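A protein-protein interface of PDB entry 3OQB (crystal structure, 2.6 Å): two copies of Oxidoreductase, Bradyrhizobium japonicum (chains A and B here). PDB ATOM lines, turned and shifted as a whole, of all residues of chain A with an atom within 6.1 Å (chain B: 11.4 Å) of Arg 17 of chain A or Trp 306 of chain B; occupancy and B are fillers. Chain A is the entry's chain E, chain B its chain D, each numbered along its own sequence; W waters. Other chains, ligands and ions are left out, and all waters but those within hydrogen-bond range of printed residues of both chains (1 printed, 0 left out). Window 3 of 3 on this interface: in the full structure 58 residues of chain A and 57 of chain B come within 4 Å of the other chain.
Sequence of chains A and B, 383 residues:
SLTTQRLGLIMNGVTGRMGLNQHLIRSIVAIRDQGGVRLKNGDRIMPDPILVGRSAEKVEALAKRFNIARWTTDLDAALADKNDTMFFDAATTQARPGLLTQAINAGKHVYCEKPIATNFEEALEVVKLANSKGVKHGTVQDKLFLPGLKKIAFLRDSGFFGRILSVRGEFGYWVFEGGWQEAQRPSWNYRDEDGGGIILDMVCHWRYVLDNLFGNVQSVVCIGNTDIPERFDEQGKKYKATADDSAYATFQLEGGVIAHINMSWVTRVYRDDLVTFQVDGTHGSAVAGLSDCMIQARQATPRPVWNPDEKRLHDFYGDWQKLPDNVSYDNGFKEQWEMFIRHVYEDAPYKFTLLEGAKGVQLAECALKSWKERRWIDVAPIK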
ATOM      1  N   THR A  15      16.177   8.833   0.062  1.00  0.00           N
ATOM      2  CA  THR A  15      15.406   9.367   1.203  1.00  0.00           C
ATOM      3  C   THR A  15      14.154   8.521   1.381  1.00  0.00           C
ATOM      4  O   THR A  15      13.865   8.054   2.479  1.00  0.00           O
ATOM      5  CB  THR A  15      15.026  10.879   1.047  1.00  0.00           C
ATOM      6  OG1 THR A  15      16.182  11.689   1.293  1.00  0.00           O
ATOM      7  CG2 THR A  15      13.900  11.291   2.004  1.00  0.00           C
ATOM      8  N   GLY A  16      13.418   8.331   0.289  1.00  0.00           N
ATOM      9  CA  GLY A  16      12.254   7.465   0.288  1.00  0.00           C
ATOM     10  C   GLY A  16      12.673   6.058   0.657  1.00  0.00           C
ATOM     11  O   GLY A  16      13.832   5.675   0.479  1.00  0.00           O
ATOM     12  N   ARG A  17      11.726   5.287   1.175  1.00  0.00           N
ATOM     13  CA  ARG A  17      12.008   3.950   1.677  1.00  0.00           C
ATOM     14  C   ARG A  17      12.780   3.116   0.640  1.00  0.00           C
ATOM     15  O   ARG A  17      13.875   2.631   0.931  1.00  0.00           O
ATOM     16  CB  ARG A  17      10.704   3.271   2.133  1.00  0.00           C
ATOM     17  CG  ARG A  17      10.813   2.425   3.413  1.00  0.00           C
ATOM     18  CD  ARG A  17      10.867   0.920   3.124  1.00  0.00           C
ATOM     19  NE  ARG A  17       9.756   0.467   2.281  1.00  0.00           N
ATOM     20  CZ  ARG A  17       9.684  -0.728   1.693  1.00  0.00           C
ATOM     21  NH1 ARG A  17      10.654  -1.621   1.856  1.00  0.00           N
ATOM     22  NH2 ARG A  17       8.638  -1.036   0.931  1.00  0.00           N
ATOM     23  N   MET A  18      12.240   2.990  -0.572  1.00  0.00           N
ATOM     24  CA  MET A  18      12.872   2.164  -1.610  1.00  0.00           C
ATOM     25  C   MET A  18      14.175   2.758  -2.143  1.00  0.00           C
ATOM     26  O   MET A  18      15.157   2.034  -2.327  1.00  0.00           O
ATOM     27  CB  MET A  18      11.902   1.867  -2.757  1.00  0.00           C
ATOM     28  CG  MET A  18      10.745   0.929  -2.380  1.00  0.00           C
ATOM     29  SD  MET A  18      11.290  -0.925  -1.957  1.00  0.00           S
ATOM     30  CE  MET A  18      11.920  -1.476  -3.743  1.00  0.00           C
ATOM     31  N   GLY A  19      14.186   4.070  -2.372  1.00  0.00           N
ATOM     32  CA  GLY A  19      15.399   4.771  -2.802  1.00  0.00           C
ATOM     33  C   GLY A  19      16.591   4.597  -1.867  1.00  0.00           C
ATOM     34  O   GLY A  19      17.693   4.261  -2.305  1.00  0.00           O
ATOM     35  N   LEU A  20      16.363   4.816  -0.574  1.00  0.00           N
ATOM     36  CA  LEU A  20      17.423   4.746   0.428  1.00  0.00           C
ATOM     37  C   LEU A  20      17.916   3.327   0.594  1.00  0.00           C
ATOM     38  O   LEU A  20      19.116   3.068   0.525  1.00  0.00           O
ATOM     39  CB  LEU A  20      16.937   5.328   1.764  1.00  0.00           C
ATOM     40  CG  LEU A  20      17.819   5.332   3.020  1.00  0.00           C
ATOM     41  CD1 LEU A  20      17.707   6.653   3.708  1.00  0.00           C
ATOM     42  CD2 LEU A  20      17.385   4.240   3.986  1.00  0.00           C
ATOM     43  N   ASN A  21      16.975   2.407   0.779  1.00  0.00           N
ATOM     44  CA  ASN A  21      17.316   1.018   1.070  1.00  0.00           C
ATOM     45  C   ASN A  21      17.967   0.269  -0.085  1.00  0.00           C
ATOM     46  O   ASN A  21      19.049  -0.274   0.072  1.00  0.00           O
ATOM     47  CB  ASN A  21      16.105   0.274   1.623  1.00  0.00           C
ATOM     48  CG  ASN A  21      15.688   0.785   3.005  1.00  0.00           C
ATOM     49  OD1 ASN A  21      16.525   0.928   3.899  1.00  0.00           O
ATOM     50  ND2 ASN A  21      14.395   1.065   3.180  1.00  0.00           N
ATOM     51  N   GLN A  22      17.333   0.279  -1.250  1.00  0.00           N
ATOM     52  CA  GLN A  22      17.826  -0.472  -2.395  1.00  0.00           C
ATOM     53  C   GLN A  22      18.985   0.185  -3.123  1.00  0.00           C
ATOM     54  O   GLN A  22      20.007  -0.448  -3.387  1.00  0.00           O
ATOM     55  CB  GLN A  22      16.681  -0.747  -3.362  1.00  0.00           C
ATOM     56  CG  GLN A  22      15.565  -1.597  -2.739  1.00  0.00           C
ATOM     57  CD  GLN A  22      16.081  -2.893  -2.091  1.00  0.00           C
ATOM     58  OE1 GLN A  22      17.056  -3.499  -2.557  1.00  0.00           O
ATOM     59  NE2 GLN A  22      15.424  -3.316  -1.014  1.00  0.00           N
ATOM     60  N   ASP A 142      14.036  -4.337 -12.033  1.00  0.00           N
ATOM     61  CA  ASP A 142      14.387  -5.182 -10.898  1.00  0.00           C
ATOM     62  C   ASP A 142      13.704  -6.552 -10.741  1.00  0.00           C
ATOM     63  O   ASP A 142      14.343  -7.502 -10.267  1.00  0.00           O
ATOM     64  CB  ASP A 142      14.231  -4.384  -9.602  1.00  0.00           C
ATOM     65  CG  ASP A 142      12.820  -3.873  -9.404  1.00  0.00           C
ATOM     66  OD1 ASP A 142      12.445  -2.860 -10.066  1.00  0.00           O
ATOM     67  OD2 ASP A 142      12.095  -4.488  -8.585  1.00  0.00           O
ATOM     68  N   LYS A 143      12.429  -6.672 -11.105  1.00  0.00           N
ATOM     69  CA  LYS A 143      11.718  -7.954 -10.948  1.00  0.00           C
ATOM     70  C   LYS A 143      12.448  -9.116 -11.613  1.00  0.00           C
ATOM     71  O   LYS A 143      12.371 -10.259 -11.162  1.00  0.00           O
ATOM     72  CB  LYS A 143      10.303  -7.877 -11.519  1.00  0.00           C
ATOM     73  CG  LYS A 143       9.221  -7.591 -10.510  1.00  0.00           C
ATOM     74  CD  LYS A 143       9.228  -6.144 -10.137  1.00  0.00           C
ATOM     75  CE  LYS A 143       8.418  -5.868  -8.878  1.00  0.00           C
ATOM     76  NZ  LYS A 143       8.895  -4.539  -8.366  1.00  0.00           N
ATOM     77  N   LEU A 146      14.927 -10.831  -9.423  1.00  0.00           N
ATOM     78  CA  LEU A 146      14.426 -11.622  -8.313  1.00  0.00           C
ATOM     79  C   LEU A 146      14.922 -13.050  -8.469  1.00  0.00           C
ATOM     80  O   LEU A 146      14.886 -13.617  -9.575  1.00  0.00           O
ATOM     81  CB  LEU A 146      12.893 -11.624  -8.253  1.00  0.00           C
ATOM     82  CG  LEU A 146      12.193 -10.317  -7.895  1.00  0.00           C
ATOM     83  CD1 LEU A 146      10.662 -10.417  -8.206  1.00  0.00           C
ATOM     84  CD2 LEU A 146      12.503  -9.850  -6.446  1.00  0.00           C
ATOM     85  N   PHE A 171      -0.359 -10.667  -7.876  1.00  0.00           N
ATOM     86  CA  PHE A 171       0.449  -9.665  -7.195  1.00  0.00           C
ATOM     87  C   PHE A 171      -0.371  -8.867  -6.208  1.00  0.00           C
ATOM     88  O   PHE A 171      -1.548  -8.557  -6.456  1.00  0.00           O
ATOM     89  CB  PHE A 171       1.119  -8.696  -8.180  1.00  0.00           C
ATOM     90  CG  PHE A 171       1.748  -7.527  -7.506  1.00  0.00           C
ATOM     91  CD1 PHE A 171       3.052  -7.609  -7.007  1.00  0.00           C
ATOM     92  CD2 PHE A 171       1.037  -6.365  -7.306  1.00  0.00           C
ATOM     93  CE1 PHE A 171       3.656  -6.509  -6.336  1.00  0.00           C
ATOM     94  CE2 PHE A 171       1.607  -5.281  -6.650  1.00  0.00           C
ATOM     95  CZ  PHE A 171       2.913  -5.350  -6.162  1.00  0.00           C
ATOM     96  N   TYR A 173      -0.973  -7.212  -1.885  1.00  0.00           N
ATOM     97  CA  TYR A 173      -1.201  -7.454  -0.459  1.00  0.00           C
ATOM     98  C   TYR A 173      -2.034  -6.301   0.080  1.00  0.00           C
ATOM     99  O   TYR A 173      -2.211  -5.291  -0.618  1.00  0.00           O
ATOM    100  CB  TYR A 173       0.120  -7.536   0.301  1.00  0.00           C
ATOM    101  CG  TYR A 173       1.097  -6.391   0.046  1.00  0.00           C
ATOM    102  CD1 TYR A 173       1.190  -5.332   0.944  1.00  0.00           C
ATOM    103  CD2 TYR A 173       1.956  -6.388  -1.072  1.00  0.00           C
ATOM    104  CE1 TYR A 173       2.076  -4.286   0.747  1.00  0.00           C
ATOM    105  CE2 TYR A 173       2.858  -5.336  -1.281  1.00  0.00           C
ATOM    106  CZ  TYR A 173       2.903  -4.288  -0.355  1.00  0.00           C
ATOM    107  OH  TYR A 173       3.784  -3.234  -0.514  1.00  0.00           O
ATOM    108  N   GLN A 184       1.296   0.974   4.445  1.00  0.00           N
ATOM    109  CA  GLN A 184       2.667   0.556   4.086  1.00  0.00           C
ATOM    110  C   GLN A 184       3.266   1.407   2.982  1.00  0.00           C
ATOM    111  O   GLN A 184       4.480   1.429   2.825  1.00  0.00           O
ATOM    112  CB  GLN A 184       2.731  -0.897   3.574  1.00  0.00           C
ATOM    113  CG  GLN A 184       2.319  -1.980   4.559  1.00  0.00           C
ATOM    114  CD  GLN A 184       0.843  -2.301   4.484  1.00  0.00           C
ATOM    115  OE1 GLN A 184      -0.018  -1.409   4.533  1.00  0.00           O
ATOM    116  NE2 GLN A 184       0.540  -3.590   4.361  1.00  0.00           N
ATOM    117  N   LEU A 274       4.463 -12.333  -1.910  1.00  0.00           N
ATOM    118  CA  LEU A 274       3.784 -11.086  -2.279  1.00  0.00           C
ATOM    119  C   LEU A 274       3.595 -10.913  -3.782  1.00  0.00           C
ATOM    120  O   LEU A 274       2.861 -10.039  -4.221  1.00  0.00           O
ATOM    121  CB  LEU A 274       4.494  -9.869  -1.701  1.00  0.00           C
ATOM    122  CG  LEU A 274       4.816  -9.822  -0.209  1.00  0.00           C
ATOM    123  CD1 LEU A 274       5.506  -8.500   0.070  1.00  0.00           C
ATOM    124  CD2 LEU A 274       3.580  -9.998   0.671  1.00  0.00           C
ATOM    125  N   VAL A 275       4.283 -11.727  -4.567  1.00  0.00           N
ATOM    126  CA  VAL A 275       3.872 -11.981  -5.933  1.00  0.00           C
ATOM    127  C   VAL A 275       4.186 -13.440  -6.251  1.00  0.00           C
ATOM    128  O   VAL A 275       5.086 -14.041  -5.669  1.00  0.00           O
ATOM    129  CB  VAL A 275       4.536 -11.053  -6.961  1.00  0.00           C
ATOM    130  CG1 VAL A 275       6.030 -11.347  -7.073  1.00  0.00           C
ATOM    131  CG2 VAL A 275       3.908 -11.250  -8.318  1.00  0.00           C
ATOM    132  N   LEU A 290       9.155 -14.412  -4.798  1.00  0.00           N
ATOM    133  CA  LEU A 290      10.317 -13.533  -4.865  1.00  0.00           C
ATOM    134  C   LEU A 290      11.588 -14.348  -4.855  1.00  0.00           C
ATOM    135  O   LEU A 290      12.516 -14.052  -5.604  1.00  0.00           O
ATOM    136  CB  LEU A 290      10.344 -12.537  -3.698  1.00  0.00           C
ATOM    137  CG  LEU A 290       9.593 -11.204  -3.804  1.00  0.00           C
ATOM    138  CD1 LEU A 290       8.085 -11.367  -3.980  1.00  0.00           C
ATOM    139  CD2 LEU A 290       9.859 -10.396  -2.562  1.00  0.00           C
ATOM    140  N   PHE A 333      19.157  -4.892  -7.443  1.00  0.00           N
ATOM    141  CA  PHE A 333      19.450  -3.493  -7.770  1.00  0.00           C
ATOM    142  C   PHE A 333      20.951  -3.300  -7.940  1.00  0.00           C
ATOM    143  O   PHE A 333      21.396  -2.819  -8.982  1.00  0.00           O
ATOM    144  CB  PHE A 333      18.873  -2.552  -6.721  1.00  0.00           C
ATOM    145  CG  PHE A 333      17.372  -2.576  -6.658  1.00  0.00           C
ATOM    146  CD1 PHE A 333      16.708  -3.457  -5.803  1.00  0.00           C
ATOM    147  CD2 PHE A 333      16.614  -1.725  -7.465  1.00  0.00           C
ATOM    148  CE1 PHE A 333      15.296  -3.485  -5.754  1.00  0.00           C
ATOM    149  CE2 PHE A 333      15.196  -1.739  -7.421  1.00  0.00           C
ATOM    150  CZ  PHE A 333      14.536  -2.621  -6.566  1.00  0.00           C
ATOM    151  N   PRO B 302      -1.804  -9.532   8.311  1.00  0.00           N
ATOM    152  CA  PRO B 302      -0.468  -9.123   8.719  1.00  0.00           C
ATOM    153  C   PRO B 302      -0.064  -7.839   7.997  1.00  0.00           C
ATOM    154  O   PRO B 302      -0.862  -7.265   7.253  1.00  0.00           O
ATOM    155  CB  PRO B 302       0.401 -10.306   8.282  1.00  0.00           C
ATOM    156  CG  PRO B 302      -0.321 -10.842   7.074  1.00  0.00           C
ATOM    157  CD  PRO B 302      -1.775 -10.647   7.347  1.00  0.00           C
ATOM    158  N   ARG B 303       1.170  -7.408   8.213  1.00  0.00           N
ATOM    159  CA  ARG B 303       1.640  -6.172   7.621  1.00  0.00           C
ATOM    160  C   ARG B 303       2.978  -6.339   6.893  1.00  0.00           C
ATOM    161  O   ARG B 303       3.942  -5.670   7.243  1.00  0.00           O
ATOM    162  CB  ARG B 303       1.745  -5.092   8.700  1.00  0.00           C
ATOM    163  CG  ARG B 303       2.042  -3.714   8.172  1.00  0.00           C
ATOM    164  CD  ARG B 303       2.734  -2.881   9.230  1.00  0.00           C
ATOM    165  NE  ARG B 303       3.250  -1.625   8.680  1.00  0.00           N
ATOM    166  CZ  ARG B 303       2.501  -0.543   8.492  1.00  0.00           C
ATOM    167  NH1 ARG B 303       3.021   0.566   7.976  1.00  0.00           N
ATOM    168  NH2 ARG B 303       1.214  -0.586   8.813  1.00  0.00           N
ATOM    169  N   PRO B 304       3.025  -7.186   5.844  1.00  0.00           N
ATOM    170  CA  PRO B 304       4.287  -7.364   5.130  1.00  0.00           C
ATOM    171  C   PRO B 304       4.630  -6.095   4.355  1.00  0.00           C
ATOM    172  O   PRO B 304       3.743  -5.273   4.059  1.00  0.00           O
ATOM    173  CB  PRO B 304       3.959  -8.474   4.151  1.00  0.00           C
ATOM    174  CG  PRO B 304       2.514  -8.159   3.774  1.00  0.00           C
ATOM    175  CD  PRO B 304       1.887  -7.738   5.075  1.00  0.00           C
ATOM    176  N   VAL B 305       5.908  -5.928   4.043  1.00  0.00           N
ATOM    177  CA  VAL B 305       6.377  -4.767   3.275  1.00  0.00           C
ATOM    178  C   VAL B 305       7.339  -5.243   2.176  1.00  0.00           C
ATOM    179  O   VAL B 305       8.146  -6.159   2.408  1.00  0.00           O
ATOM    180  CB  VAL B 305       7.008  -3.685   4.214  1.00  0.00           C
ATOM    181  CG1 VAL B 305       8.433  -4.074   4.666  1.00  0.00           C
ATOM    182  CG2 VAL B 305       6.975  -2.307   3.566  1.00  0.00           C
ATOM    183  N   TRP B 306       7.232  -4.660   0.983  1.00  0.00           N
ATOM    184  CA  TRP B 306       8.022  -5.136  -0.162  1.00  0.00           C
ATOM    185  C   TRP B 306       9.533  -5.091   0.121  1.00  0.00           C
ATOM    186  O   TRP B 306      10.088  -4.031   0.416  1.00  0.00           O
ATOM    187  CB  TRP B 306       7.670  -4.363  -1.437  1.00  0.00           C
ATOM    188  CG  TRP B 306       8.303  -4.958  -2.665  1.00  0.00           C
ATOM    189  CD1 TRP B 306       9.484  -4.585  -3.245  1.00  0.00           C
ATOM    190  CD2 TRP B 306       7.798  -6.044  -3.449  1.00  0.00           C
ATOM    191  NE1 TRP B 306       9.746  -5.372  -4.339  1.00  0.00           N
ATOM    192  CE2 TRP B 306       8.726  -6.274  -4.489  1.00  0.00           C
ATOM    193  CE3 TRP B 306       6.650  -6.837  -3.380  1.00  0.00           C
ATOM    194  CZ2 TRP B 306       8.539  -7.266  -5.449  1.00  0.00           C
ATOM    195  CZ3 TRP B 306       6.466  -7.824  -4.330  1.00  0.00           C
ATOM    196  CH2 TRP B 306       7.405  -8.030  -5.354  1.00  0.00           C
ATOM    197  N   ASN B 307      10.183  -6.253   0.047  1.00  0.00           N
ATOM    198  CA  ASN B 307      11.594  -6.386   0.445  1.00  0.00           C
ATOM    199  C   ASN B 307      12.178  -7.724  -0.012  1.00  0.00           C
ATOM    200  O   ASN B 307      11.854  -8.767   0.567  1.00  0.00           O
ATOM    201  CB  ASN B 307      11.741  -6.237   1.977  1.00  0.00           C
ATOM    202  CG  ASN B 307      13.197  -6.361   2.466  1.00  0.00           C
ATOM    203  OD1 ASN B 307      13.824  -7.428   2.386  1.00  0.00           O
ATOM    204  ND2 ASN B 307      13.720  -5.270   3.010  1.00  0.00           N
ATOM    205  N   PRO B 308      13.022  -7.705  -1.063  1.00  0.00           N
ATOM    206  CA  PRO B 308      13.775  -8.909  -1.444  1.00  0.00           C
ATOM    207  C   PRO B 308      14.918  -9.212  -0.465  1.00  0.00           C
ATOM    208  O   PRO B 308      15.760  -8.348  -0.184  1.00  0.00           O
ATOM    209  CB  PRO B 308      14.326  -8.560  -2.829  1.00  0.00           C
ATOM    210  CG  PRO B 308      13.451  -7.459  -3.326  1.00  0.00           C
ATOM    211  CD  PRO B 308      13.060  -6.675  -2.117  1.00  0.00           C
ATOM    212  N   LYS B 311      13.737 -11.424   4.090  1.00  0.00           N
ATOM    213  CA  LYS B 311      14.710 -12.514   4.028  1.00  0.00           C
ATOM    214  C   LYS B 311      14.198 -13.799   4.714  1.00  0.00           C
ATOM    215  O   LYS B 311      14.047 -14.836   4.052  1.00  0.00           O
ATOM    216  CB  LYS B 311      16.064 -12.061   4.601  1.00  0.00           C
ATOM    217  CG  LYS B 311      17.256 -12.970   4.251  1.00  0.00           C
ATOM    218  CD  LYS B 311      18.530 -12.170   3.941  1.00  0.00           C
ATOM    219  CE  LYS B 311      19.089 -11.449   5.174  1.00  0.00           C
ATOM    220  NZ  LYS B 311      20.295 -10.626   4.858  1.00  0.00           N
ATOM    221  N   ARG B 312      13.935 -13.717   6.024  1.00  0.00           N
ATOM    222  CA  ARG B 312      13.295 -14.802   6.805  1.00  0.00           C
ATOM    223  C   ARG B 312      11.950 -15.261   6.210  1.00  0.00           C
ATOM    224  O   ARG B 312      11.053 -14.440   5.967  1.00  0.00           O
ATOM    225  CB  ARG B 312      13.085 -14.361   8.271  1.00  0.00           C
ATOM    226  CG  ARG B 312      14.044 -14.982   9.302  1.00  0.00           C
ATOM    227  CD  ARG B 312      13.421 -16.206  10.008  1.00  0.00           C
ATOM    228  NE  ARG B 312      14.402 -16.962  10.802  1.00  0.00           N
ATOM    229  CZ  ARG B 312      14.411 -17.060  12.135  1.00  0.00           C
ATOM    230  NH1 ARG B 312      13.482 -16.456  12.870  1.00  0.00           N
ATOM    231  NH2 ARG B 312      15.356 -17.777  12.738  1.00  0.00           N
ATOM    232  N   PHE B 316       2.260 -17.299   4.732  1.00  0.00           N
ATOM    233  CA  PHE B 316       1.017 -16.547   4.538  1.00  0.00           C
ATOM    234  C   PHE B 316      -0.222 -17.382   4.761  1.00  0.00           C
ATOM    235  O   PHE B 316      -1.189 -16.902   5.353  1.00  0.00           O
ATOM    236  CB  PHE B 316       1.002 -15.839   3.183  1.00  0.00           C
ATOM    237  CG  PHE B 316       1.973 -14.690   3.110  1.00  0.00           C
ATOM    238  CD1 PHE B 316       3.172 -14.820   2.454  1.00  0.00           C
ATOM    239  CD2 PHE B 316       1.691 -13.499   3.756  1.00  0.00           C
ATOM    240  CE1 PHE B 316       4.070 -13.749   2.412  1.00  0.00           C
ATOM    241  CE2 PHE B 316       2.568 -12.449   3.719  1.00  0.00           C
ATOM    242  CZ  PHE B 316       3.764 -12.568   3.046  1.00  0.00           C
HETATM  243  O   HOH W   1      -1.079  -6.556   4.624  1.00  0.00           O
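The backbone carbonyl oxygen (O) of Trp 306 of chain B is in hydrogen-bond range of the guanidinium group (NH1) of Arg 17 of chain A (2.9 Å).
The backbone carbonyl oxygen (O) of Arg 17 of chain A sits at hydrogen-bond distance from the side-chain amide nitrogen (ND2) of Asn 21 of chain A, at 2.8 Å. NZ of Lys 143 of chain A is in salt-bridge range of OD2 of Asp 142 of chain A (3.2 Å).
Among the printed residues, pairs that only touch across the chains: Arg 17 of chain A with Val 305 of chain B, Leu 274 of chain A with Phe 316 of chain B, Gln 184 of chain A with Pro 304 of chain B, Leu 290 of chain A with Trp 306 of chain B, Phe 171 of chain A with Trp 306 of chain B, Lys 143 of chain A with Trp 306 of chain B, Leu 274 of chain A with Pro 304 of chain B, Tyr 173 of chain A with Pro 304 of chain B, Leu 274 of chain A with Trp 306 of chain B, Gln 184 of chain A with Arg 303 of chain B, Met 18 of chain A with Trp 306 of chain B and Val 275 of chain A with Trp 306 of chain B.
Arg 17 of chain A touches just these residues of chain B: Val 305 and Trp 306. Of the printed residues of chain A, Trp 306 of chain B touches Arg 17 (2.9 Å), Met 18 (3.98 Å), Lys 143 (3.7 Å), Phe 171 (3.7 Å), Leu 274 (3.9 Å), Val 275 (3.98 Å) and Leu 290 (3.7 Å). No residue of chain B comes within 4 Å of Gly 16 of chain A. No residue of chain B comes within 4 Å of Gly 19 of chain A. No residue of chain B comes within 4 Å of Asn 21 of chain A. Printed residues of chain A within 4 Å of Val 305 of chain B: Arg 17. Printed residues of chain A within 4 Å of Arg 303 of chain B: Gln 184 (3.9 Å). The nearest residue of chain B that does not touch Arg 17 of chain A is Asn 307 of chain B (4.7 Å).
Of the 18 printed residues of chain A, 9 touch a printed residue of chain B. Hydrophobic or aromatic side chains of chain A that line the printed part of chain B: Met 18, Phe 171, Tyr 173, Leu 274, Val 275 and Leu 290. Printed residues of chain B that touch a printed residue of chain A: Arg 303, Pro 304, Val 305, Trp 306 and Phe 316. Among the printed residues, no Asp or Glu carboxylate lies within 4 Å of a Lys or Arg side-chain nitrogen of the other chain.
No position is printed for both chains.
Water W1 bridges the backbone carbonyl oxygen (O) of Pro 302 of chain B (2.7 Å) and the side-chain amide nitrogen (NE2) of Gln 184 of chain A (3.4 Å).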
